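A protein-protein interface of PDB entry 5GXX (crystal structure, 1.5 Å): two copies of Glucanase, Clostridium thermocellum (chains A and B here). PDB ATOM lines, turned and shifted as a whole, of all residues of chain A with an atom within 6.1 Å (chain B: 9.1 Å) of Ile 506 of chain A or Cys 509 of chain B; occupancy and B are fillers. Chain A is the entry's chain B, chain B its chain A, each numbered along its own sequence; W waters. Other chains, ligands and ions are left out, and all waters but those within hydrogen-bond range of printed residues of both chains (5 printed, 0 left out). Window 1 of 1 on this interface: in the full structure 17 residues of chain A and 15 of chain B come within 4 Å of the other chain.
The side-chain sulfur (SG) of Cys 509 of chain B sits close to the backbone NH (N) of Tyr 508 of chain A.
SG of Cys 509 of chain B forms a disulfide with SG of Cys 509 of chain A (2.1 Å).
The backbone NH (N) of Gly 512 of chain B lies within hydrogen-bond range of the backbone carbonyl oxygen (O) of Gly 507 of chain A.
The side-chain hydroxyl of Thr 505 of chain A sits at hydrogen-bond distance from the side-chain carboxylate of Asp 514 of chain B, 2.4 Å away.
OD2 of Asp 514 of chain B is in salt-bridge range of NH1 of Arg 555 of chain A.
The backbone carbonyl oxygen of Ile 506 of chain A sits at hydrogen-bond distance from the backbone NH of Val 515 of chain B, at 2.9 Å.
O of Ile 506 of chain A lies close to O of Met 513 of chain B (3.3 Å).
The backbone carbonyl oxygen (O) of Gly 507 of chain A lies close to the backbone carbonyl oxygen (O) of Glu 510 of chain B (3.4 Å).
N of Gln 553 of chain B lies within hydrogen-bond range of O of Tyr 508 of chain B, 2.9 Å away.
The backbone NH (N) of Gln 553 of chain A sits at hydrogen-bond distance from the backbone carbonyl oxygen (O) of Tyr 508 of chain A (2.9 Å).
O of Val 515 of chain B touches CB of Thr 505 of chain A (3.3 Å).
Thr 505 of chain A touches Ile 535 of chain B (CG2 to CG1, 3.9 Å).
O of Gly 507 of chain A touches CA of Ser 511 of chain B (3.3 Å).
N of Met 513 of chain B touches O of Gly 507 of chain A (3.8 Å).
Tyr 508 of chain A touches Ser 511 of chain B.
Of chain B, only Cys 509, Met 513, Asp 514 and Val 515 come within 4 Å of Ile 506 of chain A.
Of the printed residues of chain A, Cys 509 of chain B touches Ile 506, Tyr 508 and Cys 509.
Of chain B, only Glu 510, Ser 511, Gly 512 and Met 513 come within 4 Å of Gly 507 of chain A.
Cys 509 of chain A touches three residues of chain B.
Printed residues of chain A within 4 Å of Ile 535 of chain B: Thr 505 (3.9 Å).
Of the printed residues of chain B, Ser 511 of chain A touches Gly 507 (3.5 Å) and Tyr 508 (3.7 Å).
The nearest residue of chain B that does not touch Ile 506 of chain A is Ile 506 of chain B (5.0 Å).
The nearest printed residue of chain A that does not touch Ile 506 of chain B is Ile 506 of chain A (5.0 Å).
Of the 13 printed residues of chain A, 9 touch a printed residue of chain B.
Printed residues of chain A that touch a printed residue of chain B: Val 504, Thr 505, Ile 506, Gly 507, Tyr 508, Cys 509, Glu 510, Ser 511 and Arg 555.
Hydrophobic or aromatic side chains of chain A that line the printed part of chain B: Ile 506 and Tyr 508.
Of the 25 printed residues of chain B, 12 touch a printed residue of chain A.
Ile 506 of chain A touches Cys 509 of chain B, and with the chains exchanged Cys 509 of chain A touches Ile 506 of chain B.
Gly 507 of chain A touches Ser 511 of chain B, and with the chains exchanged Ser 511 of chain A touches Gly 507 of chain B.
Water W1 bridges the side-chain hydroxyl of Ser 511 of chain A (2.8 Å) and the side-chain amide nitrogen of Gln 553 of chain B (3.1 Å).
Water W4 bridges the side-chain hydroxyl (OG) of Ser 511 of chain B and the side-chain amide nitrogen (NE2) of Gln 553 of chain A.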
ATOM      1  N   VAL A 504      16.881  24.798 -15.117  1.00  0.00           N
ATOM      2  CA  VAL A 504      17.920  23.819 -14.774  1.00  0.00           C
ATOM      3  C   VAL A 504      19.278  24.505 -14.839  1.00  0.00           C
ATOM      4  O   VAL A 504      19.673  25.031 -15.890  1.00  0.00           O
ATOM      5  CB  VAL A 504      17.903  22.599 -15.717  1.00  0.00           C
ATOM      6  CG1 VAL A 504      18.906  21.531 -15.275  1.00  0.00           C
ATOM      7  CG2 VAL A 504      16.509  21.979 -15.789  1.00  0.00           C
ATOM      8  N   THR A 505      20.006  24.468 -13.723  1.00  0.00           N
ATOM      9  CA  THR A 505      21.371  25.010 -13.685  1.00  0.00           C
ATOM     10  C   THR A 505      22.366  24.037 -13.058  1.00  0.00           C
ATOM     11  O   THR A 505      21.966  23.029 -12.458  1.00  0.00           O
ATOM     12  CB  THR A 505      21.445  26.339 -12.908  1.00  0.00           C
ATOM     13  OG1 THR A 505      20.964  26.139 -11.576  1.00  0.00           O
ATOM     14  CG2 THR A 505      20.615  27.422 -13.605  1.00  0.00           C
ATOM     15  N   ILE A 506      23.651  24.337 -13.219  1.00  0.00           N
ATOM     16  CA  ILE A 506      24.707  23.535 -12.610  1.00  0.00           C
ATOM     17  C   ILE A 506      25.537  24.397 -11.667  1.00  0.00           C
ATOM     18  O   ILE A 506      25.847  25.554 -11.972  1.00  0.00           O
ATOM     19  CB  ILE A 506      25.625  22.912 -13.683  1.00  0.00           C
ATOM     20  CG1 ILE A 506      24.893  21.829 -14.476  1.00  0.00           C
ATOM     21  CG2 ILE A 506      26.817  22.269 -13.011  1.00  0.00           C
ATOM     22  CD1 ILE A 506      24.234  20.818 -13.591  1.00  0.00           C
ATOM     23  N   GLY A 507      25.906  23.817 -10.530  1.00  0.00           N
ATOM     24  CA  GLY A 507      26.766  24.478  -9.553  1.00  0.00           C
ATOM     25  C   GLY A 507      28.154  23.912  -9.343  1.00  0.00           C
ATOM     26  O   GLY A 507      28.964  24.530  -8.658  1.00  0.00           O
ATOM     27  N   TYR A 508      28.400  22.747  -9.936  1.00  0.00           N
ATOM     28  CA  TYR A 508      29.707  22.097  -9.962  1.00  0.00           C
ATOM     29  C   TYR A 508      29.639  20.946 -10.960  1.00  0.00           C
ATOM     30  O   TYR A 508      28.700  20.152 -10.956  1.00  0.00           O
ATOM     31  CB  TYR A 508      30.116  21.564  -8.586  1.00  0.00           C
ATOM     32  CG  TYR A 508      31.413  20.782  -8.606  1.00  0.00           C
ATOM     33  CD1 TYR A 508      32.614  21.395  -8.951  1.00  0.00           C
ATOM     34  CD2 TYR A 508      31.432  19.416  -8.353  1.00  0.00           C
ATOM     35  CE1 TYR A 508      33.798  20.677  -8.994  1.00  0.00           C
ATOM     36  CE2 TYR A 508      32.619  18.702  -8.376  1.00  0.00           C
ATOM     37  CZ  TYR A 508      33.795  19.330  -8.715  1.00  0.00           C
ATOM     38  OH  TYR A 508      34.965  18.588  -8.746  1.00  0.00           O
ATOM     39  N   CYS A 509      30.653  20.875 -11.813  1.00  0.00           N
ATOM     40  CA  CYS A 509      30.786  19.796 -12.795  1.00  0.00           C
ATOM     41  C   CYS A 509      32.249  19.375 -12.696  1.00  0.00           C
ATOM     42  O   CYS A 509      33.141  20.138 -13.068  1.00  0.00           O
ATOM     43  CB  CYS A 509      30.494  20.309 -14.219  1.00  0.00           C
ATOM     44  SG  CYS A 509      29.086  21.455 -14.390  1.00  0.00           S
ATOM     45  N   GLU A 510      32.489  18.155 -12.223  1.00  0.00           N
ATOM     46  CA  GLU A 510      33.848  17.656 -12.051  1.00  0.00           C
ATOM     47  C   GLU A 510      34.643  17.709 -13.352  1.00  0.00           C
ATOM     48  O   GLU A 510      34.152  17.293 -14.412  1.00  0.00           O
ATOM     49  CB  GLU A 510      33.799  16.223 -11.511  1.00  0.00           C
ATOM     50  CG  GLU A 510      35.179  15.668 -11.167  1.00  0.00           C
ATOM     51  CD  GLU A 510      35.104  14.277 -10.601  1.00  0.00           C
ATOM     52  OE1 GLU A 510      34.025  13.880 -10.122  1.00  0.00           O
ATOM     53  OE2 GLU A 510      36.140  13.579 -10.617  1.00  0.00           O
ATOM     54  N   SER A 511      35.878  18.201 -13.253  1.00  0.00           N
ATOM     55  CA  SER A 511      36.771  18.345 -14.396  1.00  0.00           C
ATOM     56  C   SER A 511      37.021  16.992 -15.049  1.00  0.00           C
ATOM     57  O   SER A 511      37.253  15.996 -14.358  1.00  0.00           O
ATOM     58  CB  SER A 511      38.096  18.957 -13.940  1.00  0.00           C
ATOM     59  OG  SER A 511      38.952  19.196 -15.046  1.00  0.00           O
ATOM     60  N   ILE A 517      23.021  17.746 -19.592  1.00  0.00           N
ATOM     61  CA  ILE A 517      21.761  17.540 -18.912  1.00  0.00           C
ATOM     62  C   ILE A 517      20.679  17.862 -19.942  1.00  0.00           C
ATOM     63  O   ILE A 517      20.705  18.920 -20.565  1.00  0.00           O
ATOM     64  CB  ILE A 517      21.633  18.472 -17.687  1.00  0.00           C
ATOM     65  CG1 ILE A 517      22.842  18.309 -16.757  1.00  0.00           C
ATOM     66  CG2 ILE A 517      20.348  18.207 -16.916  1.00  0.00           C
ATOM     67  CD1 ILE A 517      22.625  18.992 -15.428  1.00  0.00           C
ATOM     68  N   LEU A 552      28.383  15.759  -9.910  1.00  0.00           N
ATOM     69  CA  LEU A 552      27.653  16.893 -10.462  1.00  0.00           C
ATOM     70  C   LEU A 552      26.769  17.501  -9.377  1.00  0.00           C
ATOM     71  O   LEU A 552      26.134  16.790  -8.598  1.00  0.00           O
ATOM     72  CB  LEU A 552      26.801  16.410 -11.640  1.00  0.00           C
ATOM     73  CG  LEU A 552      26.051  17.478 -12.454  1.00  0.00           C
ATOM     74  CD1 LEU A 552      26.964  18.391 -13.264  1.00  0.00           C
ATOM     75  CD2 LEU A 552      25.084  16.817 -13.423  1.00  0.00           C
ATOM     76  N   GLN A 553      26.758  18.827  -9.302  1.00  0.00           N
ATOM     77  CA  GLN A 553      25.761  19.512  -8.493  1.00  0.00           C
ATOM     78  C   GLN A 553      24.816  20.203  -9.459  1.00  0.00           C
ATOM     79  O   GLN A 553      25.260  21.001 -10.284  1.00  0.00           O
ATOM     80  CB  GLN A 553      26.418  20.517  -7.542  1.00  0.00           C
ATOM     81  CG  GLN A 553      27.257  19.814  -6.481  1.00  0.00           C
ATOM     82  CD  GLN A 553      28.227  20.728  -5.754  1.00  0.00           C
ATOM     83  OE1 GLN A 553      27.976  21.928  -5.558  1.00  0.00           O
ATOM     84  NE2 GLN A 553      29.341  20.146  -5.329  1.00  0.00           N
ATOM     85  N   PHE A 554      23.537  19.835  -9.393  1.00  0.00           N
ATOM     86  CA  PHE A 554      22.533  20.441 -10.247  1.00  0.00           C
ATOM     87  C   PHE A 554      21.394  21.016  -9.424  1.00  0.00           C
ATOM     88  O   PHE A 554      21.103  20.544  -8.322  1.00  0.00           O
ATOM     89  CB  PHE A 554      22.036  19.482 -11.325  1.00  0.00           C
ATOM     90  CG  PHE A 554      21.386  18.231 -10.812  1.00  0.00           C
ATOM     91  CD1 PHE A 554      20.013  18.167 -10.612  1.00  0.00           C
ATOM     92  CD2 PHE A 554      22.141  17.090 -10.598  1.00  0.00           C
ATOM     93  CE1 PHE A 554      19.407  16.992 -10.172  1.00  0.00           C
ATOM     94  CE2 PHE A 554      21.544  15.917 -10.147  1.00  0.00           C
ATOM     95  CZ  PHE A 554      20.179  15.864  -9.936  1.00  0.00           C
ATOM     96  N   ARG A 555      20.811  22.089  -9.952  1.00  0.00           N
ATOM     97  CA  ARG A 555      19.748  22.816  -9.271  1.00  0.00           C
ATOM     98  C   ARG A 555      18.546  22.921 -10.203  1.00  0.00           C
ATOM     99  O   ARG A 555      18.689  23.147 -11.409  1.00  0.00           O
ATOM    100  CB  ARG A 555      20.233  24.199  -8.832  1.00  0.00           C
ATOM    101  CG  ARG A 555      19.174  25.034  -8.103  1.00  0.00           C
ATOM    102  CD  ARG A 555      19.648  26.457  -7.802  1.00  0.00           C
ATOM    103  NE  ARG A 555      20.683  26.467  -6.769  1.00  0.00           N
ATOM    104  CZ  ARG A 555      21.068  27.553  -6.103  1.00  0.00           C
ATOM    105  NH1 ARG A 555      20.478  28.719  -6.346  1.00  0.00           N
ATOM    106  NH2 ARG A 555      22.011  27.481  -5.168  1.00  0.00           N
ATOM    107  N   ALA B 465      36.725  29.151 -20.433  1.00  0.00           N
ATOM    108  CA  ALA B 465      36.371  30.568 -20.307  1.00  0.00           C
ATOM    109  C   ALA B 465      36.265  31.009 -18.846  1.00  0.00           C
ATOM    110  O   ALA B 465      35.627  30.353 -18.031  1.00  0.00           O
ATOM    111  CB  ALA B 465      35.069  30.832 -21.042  1.00  0.00           C
ATOM    112  N   TYR B 483      27.716  36.006 -20.772  1.00  0.00           N
ATOM    113  CA  TYR B 483      28.517  36.282 -21.946  1.00  0.00           C
ATOM    114  C   TYR B 483      28.084  35.379 -23.092  1.00  0.00           C
ATOM    115  O   TYR B 483      27.476  34.322 -22.872  1.00  0.00           O
ATOM    116  CB  TYR B 483      30.018  36.159 -21.653  1.00  0.00           C
ATOM    117  CG  TYR B 483      30.499  34.783 -21.224  1.00  0.00           C
ATOM    118  CD1 TYR B 483      30.782  33.808 -22.178  1.00  0.00           C
ATOM    119  CD2 TYR B 483      30.690  34.471 -19.882  1.00  0.00           C
ATOM    120  CE1 TYR B 483      31.254  32.567 -21.807  1.00  0.00           C
ATOM    121  CE2 TYR B 483      31.177  33.224 -19.496  1.00  0.00           C
ATOM    122  CZ  TYR B 483      31.444  32.280 -20.469  1.00  0.00           C
ATOM    123  OH  TYR B 483      31.904  31.030 -20.112  1.00  0.00           O
ATOM    124  N   THR B 505      28.074  20.499 -24.522  1.00  0.00           N
ATOM    125  CA  THR B 505      28.320  19.762 -23.295  1.00  0.00           C
ATOM    126  C   THR B 505      29.296  20.566 -22.443  1.00  0.00           C
ATOM    127  O   THR B 505      29.869  21.569 -22.895  1.00  0.00           O
ATOM    128  CB  THR B 505      28.919  18.370 -23.564  1.00  0.00           C
ATOM    129  OG1 THR B 505      30.142  18.511 -24.289  1.00  0.00           O
ATOM    130  CG2 THR B 505      27.957  17.486 -24.355  1.00  0.00           C
ATOM    131  N   ILE B 506      29.471  20.113 -21.204  1.00  0.00           N
ATOM    132  CA  ILE B 506      30.319  20.809 -20.235  1.00  0.00           C
ATOM    133  C   ILE B 506      31.377  19.824 -19.762  1.00  0.00           C
ATOM    134  O   ILE B 506      31.056  18.681 -19.428  1.00  0.00           O
ATOM    135  CB  ILE B 506      29.478  21.337 -19.054  1.00  0.00           C
ATOM    136  CG1 ILE B 506      28.573  22.476 -19.527  1.00  0.00           C
ATOM    137  CG2 ILE B 506      30.335  21.878 -17.918  1.00  0.00           C
ATOM    138  CD1 ILE B 506      27.561  22.949 -18.493  1.00  0.00           C
ATOM    139  N   GLY B 507      32.623  20.283 -19.735  1.00  0.00           N
ATOM    140  CA  GLY B 507      33.748  19.478 -19.284  1.00  0.00           C
ATOM    141  C   GLY B 507      34.267  19.866 -17.915  1.00  0.00           C
ATOM    142  O   GLY B 507      35.036  19.106 -17.329  1.00  0.00           O
ATOM    143  N   TYR B 508      33.896  21.055 -17.432  1.00  0.00           N
ATOM    144  CA  TYR B 508      34.214  21.492 -16.061  1.00  0.00           C
ATOM    145  C   TYR B 508      33.380  22.726 -15.756  1.00  0.00           C
ATOM    146  O   TYR B 508      33.209  23.602 -16.609  1.00  0.00           O
ATOM    147  CB  TYR B 508      35.691  21.856 -15.866  1.00  0.00           C
ATOM    148  CG  TYR B 508      36.032  22.536 -14.547  1.00  0.00           C
ATOM    149  CD1 TYR B 508      35.930  21.876 -13.320  1.00  0.00           C
ATOM    150  CD2 TYR B 508      36.485  23.850 -14.541  1.00  0.00           C
ATOM    151  CE1 TYR B 508      36.246  22.515 -12.121  1.00  0.00           C
ATOM    152  CE2 TYR B 508      36.814  24.502 -13.356  1.00  0.00           C
ATOM    153  CZ  TYR B 508      36.698  23.822 -12.154  1.00  0.00           C
ATOM    154  OH  TYR B 508      37.028  24.446 -10.982  1.00  0.00           O
ATOM    155  N   CYS B 509      32.848  22.789 -14.541  1.00  0.00           N
ATOM    156  CA  CYS B 509      32.215  24.033 -14.114  1.00  0.00           C
ATOM    157  C   CYS B 509      32.528  24.252 -12.643  1.00  0.00           C
ATOM    158  O   CYS B 509      32.333  23.379 -11.804  1.00  0.00           O
ATOM    159  CB  CYS B 509      30.733  24.102 -14.463  1.00  0.00           C
ATOM    160  SG  CYS B 509      29.593  23.204 -13.430  1.00  0.00           S
ATOM    161  N   GLU B 510      33.085  25.423 -12.361  1.00  0.00           N
ATOM    162  CA  GLU B 510      33.659  25.731 -11.057  1.00  0.00           C
ATOM    163  C   GLU B 510      32.633  25.694  -9.930  1.00  0.00           C
ATOM    164  O   GLU B 510      31.526  26.242 -10.060  1.00  0.00           O
ATOM    165  CB  GLU B 510      34.270  27.127 -11.124  1.00  0.00           C
ATOM    166  CG  GLU B 510      35.024  27.484  -9.880  1.00  0.00           C
ATOM    167  CD  GLU B 510      35.676  28.838  -9.964  1.00  0.00           C
ATOM    168  OE1 GLU B 510      36.030  29.266 -11.083  1.00  0.00           O
ATOM    169  OE2 GLU B 510      35.854  29.434  -8.882  1.00  0.00           O
ATOM    170  N   SER B 511      33.014  25.070  -8.817  1.00  0.00           N
ATOM    171  CA  SER B 511      32.117  24.937  -7.674  1.00  0.00           C
ATOM    172  C   SER B 511      31.588  26.266  -7.120  1.00  0.00           C
ATOM    173  O   SER B 511      32.351  27.208  -6.918  1.00  0.00           O
ATOM    174  CB  SER B 511      32.829  24.172  -6.559  1.00  0.00           C
ATOM    175  OG  SER B 511      31.940  23.930  -5.488  1.00  0.00           O
ATOM    176  N   GLY B 512      30.287  26.296  -6.843  1.00  0.00           N
ATOM    177  CA  GLY B 512      29.602  27.440  -6.251  1.00  0.00           C
ATOM    178  C   GLY B 512      29.205  28.536  -7.218  1.00  0.00           C
ATOM    179  O   GLY B 512      28.768  29.613  -6.808  1.00  0.00           O
ATOM    180  N   MET B 513      29.387  28.285  -8.509  1.00  0.00           N
ATOM    181  CA  MET B 513      29.020  29.256  -9.536  1.00  0.00           C
ATOM    182  C   MET B 513      27.816  28.721 -10.315  1.00  0.00           C
ATOM    183  O   MET B 513      27.978  28.035 -11.331  1.00  0.00           O
ATOM    184  CB  MET B 513      30.215  29.592 -10.435  1.00  0.00           C
ATOM    185  CG  MET B 513      31.430  30.163  -9.698  1.00  0.00           C
ATOM    186  SD  MET B 513      31.078  31.773  -8.952  1.00  0.00           S
ATOM    187  CE  MET B 513      32.713  32.273  -8.386  1.00  0.00           C
ATOM    188  N   ASP B 514      26.613  28.984  -9.798  1.00  0.00           N
ATOM    189  CA  ASP B 514      25.355  28.529 -10.405  1.00  0.00           C
ATOM    190  C   ASP B 514      25.253  29.095 -11.827  1.00  0.00           C
ATOM    191  O   ASP B 514      25.218  30.320 -11.993  1.00  0.00           O
ATOM    192  CB  ASP B 514      24.187  29.007  -9.525  1.00  0.00           C
ATOM    193  CG  ASP B 514      22.833  28.414  -9.914  1.00  0.00           C
ATOM    194  OD1 ASP B 514      22.731  27.213 -10.267  1.00  0.00           O
ATOM    195  OD2 ASP B 514      21.828  29.157  -9.825  1.00  0.00           O
ATOM    196  N   VAL B 515      25.222  28.227 -12.844  1.00  0.00           N
ATOM    197  CA  VAL B 515      25.359  28.645 -14.234  1.00  0.00           C
ATOM    198  C   VAL B 515      24.405  27.881 -15.156  1.00  0.00           C
ATOM    199  O   VAL B 515      24.081  26.718 -14.919  1.00  0.00           O
ATOM    200  CB  VAL B 515      26.818  28.458 -14.716  1.00  0.00           C
ATOM    201  CG1 VAL B 515      27.212  26.985 -14.723  1.00  0.00           C
ATOM    202  CG2 VAL B 515      27.074  29.080 -16.084  1.00  0.00           C
ATOM    203  N   GLU B 516      23.950  28.547 -16.209  1.00  0.00           N
ATOM    204  CA  GLU B 516      23.223  27.877 -17.279  1.00  0.00           C
ATOM    205  C   GLU B 516      23.819  28.246 -18.634  1.00  0.00           C
ATOM    206  O   GLU B 516      24.435  29.307 -18.792  1.00  0.00           O
ATOM    207  CB  GLU B 516      21.718  28.141 -17.209  1.00  0.00           C
ATOM    208  CG  GLU B 516      21.370  29.611 -17.317  1.00  0.00           C
ATOM    209  CD  GLU B 516      19.903  29.907 -17.597  1.00  0.00           C
ATOM    210  OE1 GLU B 516      19.137  29.012 -18.023  1.00  0.00           O
ATOM    211  OE2 GLU B 516      19.523  31.082 -17.407  1.00  0.00           O
ATOM    212  N   ILE B 517      23.683  27.327 -19.583  1.00  0.00           N
ATOM    213  CA  ILE B 517      24.072  27.573 -20.967  1.00  0.00           C
ATOM    214  C   ILE B 517      22.814  27.477 -21.807  1.00  0.00           C
ATOM    215  O   ILE B 517      22.067  26.505 -21.700  1.00  0.00           O
ATOM    216  CB  ILE B 517      25.135  26.584 -21.504  1.00  0.00           C
ATOM    217  CG1 ILE B 517      26.349  26.503 -20.570  1.00  0.00           C
ATOM    218  CG2 ILE B 517      25.562  27.012 -22.912  1.00  0.00           C
ATOM    219  CD1 ILE B 517      27.429  25.542 -21.048  1.00  0.00           C
ATOM    220  N   ILE B 532      26.122  32.057 -21.849  1.00  0.00           N
ATOM    221  CA  ILE B 532      26.487  31.475 -20.557  1.00  0.00           C
ATOM    222  C   ILE B 532      26.050  32.500 -19.514  1.00  0.00           C
ATOM    223  O   ILE B 532      26.536  33.630 -19.540  1.00  0.00           O
ATOM    224  CB  ILE B 532      28.022  31.244 -20.472  1.00  0.00           C
ATOM    225  CG1 ILE B 532      28.544  30.149 -21.428  1.00  0.00           C
ATOM    226  CG2 ILE B 532      28.426  30.851 -19.068  1.00  0.00           C
ATOM    227  CD1 ILE B 532      28.353  30.411 -22.912  1.00  0.00           C
ATOM    228  N   SER B 533      25.118  32.128 -18.636  1.00  0.00           N
ATOM    229  CA  SER B 533      24.566  33.035 -17.624  1.00  0.00           C
ATOM    230  C   SER B 533      24.887  32.566 -16.208  1.00  0.00           C
ATOM    231  O   SER B 533      24.667  31.396 -15.881  1.00  0.00           O
ATOM    232  CB  SER B 533      23.037  33.127 -17.757  1.00  0.00           C
ATOM    233  OG  SER B 533      22.680  33.668 -19.020  1.00  0.00           O
ATOM    234  N   TYR B 534      25.374  33.461 -15.353  1.00  0.00           N
ATOM    235  CA  TYR B 534      25.580  33.149 -13.942  1.00  0.00           C
ATOM    236  C   TYR B 534      24.422  33.761 -13.196  1.00  0.00           C
ATOM    237  O   TYR B 534      24.216  34.979 -13.242  1.00  0.00           O
ATOM    238  CB  TYR B 534      26.916  33.675 -13.421  1.00  0.00           C
ATOM    239  CG  TYR B 534      28.032  32.824 -13.968  1.00  0.00           C
ATOM    240  CD1 TYR B 534      28.398  31.643 -13.329  1.00  0.00           C
ATOM    241  CD2 TYR B 534      28.675  33.167 -15.153  1.00  0.00           C
ATOM    242  CE1 TYR B 534      29.408  30.839 -13.846  1.00  0.00           C
ATOM    243  CE2 TYR B 534      29.686  32.372 -15.683  1.00  0.00           C
ATOM    244  CZ  TYR B 534      30.039  31.204 -15.028  1.00  0.00           C
ATOM    245  OH  TYR B 534      31.047  30.417 -15.540  1.00  0.00           O
ATOM    246  N   ILE B 535      23.646  32.898 -12.557  1.00  0.00           N
ATOM    247  CA  ILE B 535      22.365  33.294 -11.988  1.00  0.00           C
ATOM    248  C   ILE B 535      22.587  34.233 -10.807  1.00  0.00           C
ATOM    249  O   ILE B 535      21.871  35.232 -10.657  1.00  0.00           O
ATOM    250  CB  ILE B 535      21.547  32.061 -11.562  1.00  0.00           C
ATOM    251  CG1 ILE B 535      21.165  31.178 -12.763  1.00  0.00           C
ATOM    252  CG2 ILE B 535      20.337  32.475 -10.731  1.00  0.00           C
ATOM    253  CD1 ILE B 535      20.513  31.874 -13.941  1.00  0.00           C
ATOM    254  N   ASP B 536      23.593  33.937  -9.991  1.00  0.00           N
ATOM    255  CA  ASP B 536      24.021  34.916  -9.001  1.00  0.00           C
ATOM    256  C   ASP B 536      25.437  35.382  -9.280  1.00  0.00           C
ATOM    257  O   ASP B 536      26.401  34.964  -8.626  1.00  0.00           O
ATOM    258  CB  ASP B 536      23.885  34.384  -7.574  1.00  0.00           C
ATOM    259  CG  ASP B 536      24.199  35.439  -6.520  1.00  0.00           C
ATOM    260  OD1 ASP B 536      24.447  36.617  -6.875  1.00  0.00           O
ATOM    261  OD2 ASP B 536      24.252  35.066  -5.330  1.00  0.00           O
ATOM    262  N   ALA B 550      34.856  33.173 -12.699  1.00  0.00           N
ATOM    263  CA  ALA B 550      34.273  31.838 -12.763  1.00  0.00           C
ATOM    264  C   ALA B 550      34.702  31.092 -14.029  1.00  0.00           C
ATOM    265  O   ALA B 550      34.573  31.626 -15.143  1.00  0.00           O
ATOM    266  CB  ALA B 550      32.762  31.945 -12.674  1.00  0.00           C
ATOM    267  N   GLU B 551      35.232  29.878 -13.849  1.00  0.00           N
ATOM    268  CA  GLU B 551      35.713  29.042 -14.943  1.00  0.00           C
ATOM    269  C   GLU B 551      34.650  28.060 -15.406  1.00  0.00           C
ATOM    270  O   GLU B 551      34.014  27.391 -14.587  1.00  0.00           O
ATOM    271  CB  GLU B 551      36.991  28.297 -14.554  1.00  0.00           C
ATOM    272  CG  GLU B 551      37.504  27.371 -15.654  1.00  0.00           C
ATOM    273  CD  GLU B 551      38.849  26.739 -15.339  1.00  0.00           C
ATOM    274  OE1 GLU B 551      39.578  27.236 -14.453  1.00  0.00           O
ATOM    275  OE2 GLU B 551      39.187  25.731 -15.993  1.00  0.00           O
ATOM    276  N   LEU B 552      34.449  28.026 -16.720  1.00  0.00           N
ATOM    277  CA  LEU B 552      33.617  27.015 -17.371  1.00  0.00           C
ATOM    278  C   LEU B 552      34.396  26.443 -18.558  1.00  0.00           C
ATOM    279  O   LEU B 552      35.079  27.186 -19.276  1.00  0.00           O
ATOM    280  CB  LEU B 552      32.327  27.679 -17.873  1.00  0.00           C
ATOM    281  CG  LEU B 552      31.293  26.770 -18.553  1.00  0.00           C
ATOM    282  CD1 LEU B 552      30.700  25.778 -17.587  1.00  0.00           C
ATOM    283  CD2 LEU B 552      30.173  27.625 -19.142  1.00  0.00           C
ATOM    284  N   GLN B 553      34.295  25.131 -18.771  1.00  0.00           N
ATOM    285  CA  GLN B 553      34.817  24.506 -19.984  1.00  0.00           C
ATOM    286  C   GLN B 553      33.608  23.958 -20.709  1.00  0.00           C
ATOM    287  O   GLN B 553      32.889  23.109 -20.182  1.00  0.00           O
ATOM    288  CB  GLN B 553      35.833  23.399 -19.679  1.00  0.00           C
ATOM    289  CG  GLN B 553      37.162  23.941 -19.152  1.00  0.00           C
ATOM    290  CD  GLN B 553      38.022  22.893 -18.486  1.00  0.00           C
ATOM    291  OE1 GLN B 553      38.011  21.723 -18.872  1.00  0.00           O
ATOM    292  NE2 GLN B 553      38.798  23.316 -17.491  1.00  0.00           N
ATOM    293  N   PHE B 554      33.354  24.475 -21.904  1.00  0.00           N
ATOM    294  CA  PHE B 554      32.218  23.992 -22.677  1.00  0.00           C
ATOM    295  C   PHE B 554      32.679  23.502 -24.034  1.00  0.00           C
ATOM    296  O   PHE B 554      33.678  23.983 -24.577  1.00  0.00           O
ATOM    297  CB  PHE B 554      31.113  25.051 -22.782  1.00  0.00           C
ATOM    298  CG  PHE B 554      31.538  26.345 -23.430  1.00  0.00           C
ATOM    299  CD1 PHE B 554      31.451  26.513 -24.801  1.00  0.00           C
ATOM    300  CD2 PHE B 554      31.980  27.412 -22.656  1.00  0.00           C
ATOM    301  CE1 PHE B 554      31.804  27.712 -25.401  1.00  0.00           C
ATOM    302  CE2 PHE B 554      32.350  28.616 -23.244  1.00  0.00           C
ATOM    303  CZ  PHE B 554      32.262  28.774 -24.617  1.00  0.00           C
HETATM  304  O   HOH W   1      40.531  21.438 -15.720  1.00  0.00           O
HETATM  305  O   HOH W   2      22.098  31.167  -7.947  1.00  0.00           O
HETATM  306  O   HOH W   3      38.344  19.231 -17.727  1.00  0.00           O
HETATM  307  O   HOH W   4      31.396  21.645  -3.894  1.00  0.00           O
HETATM  308  O   HOH W   5      18.709  26.339 -17.899  1.00  0.00           O
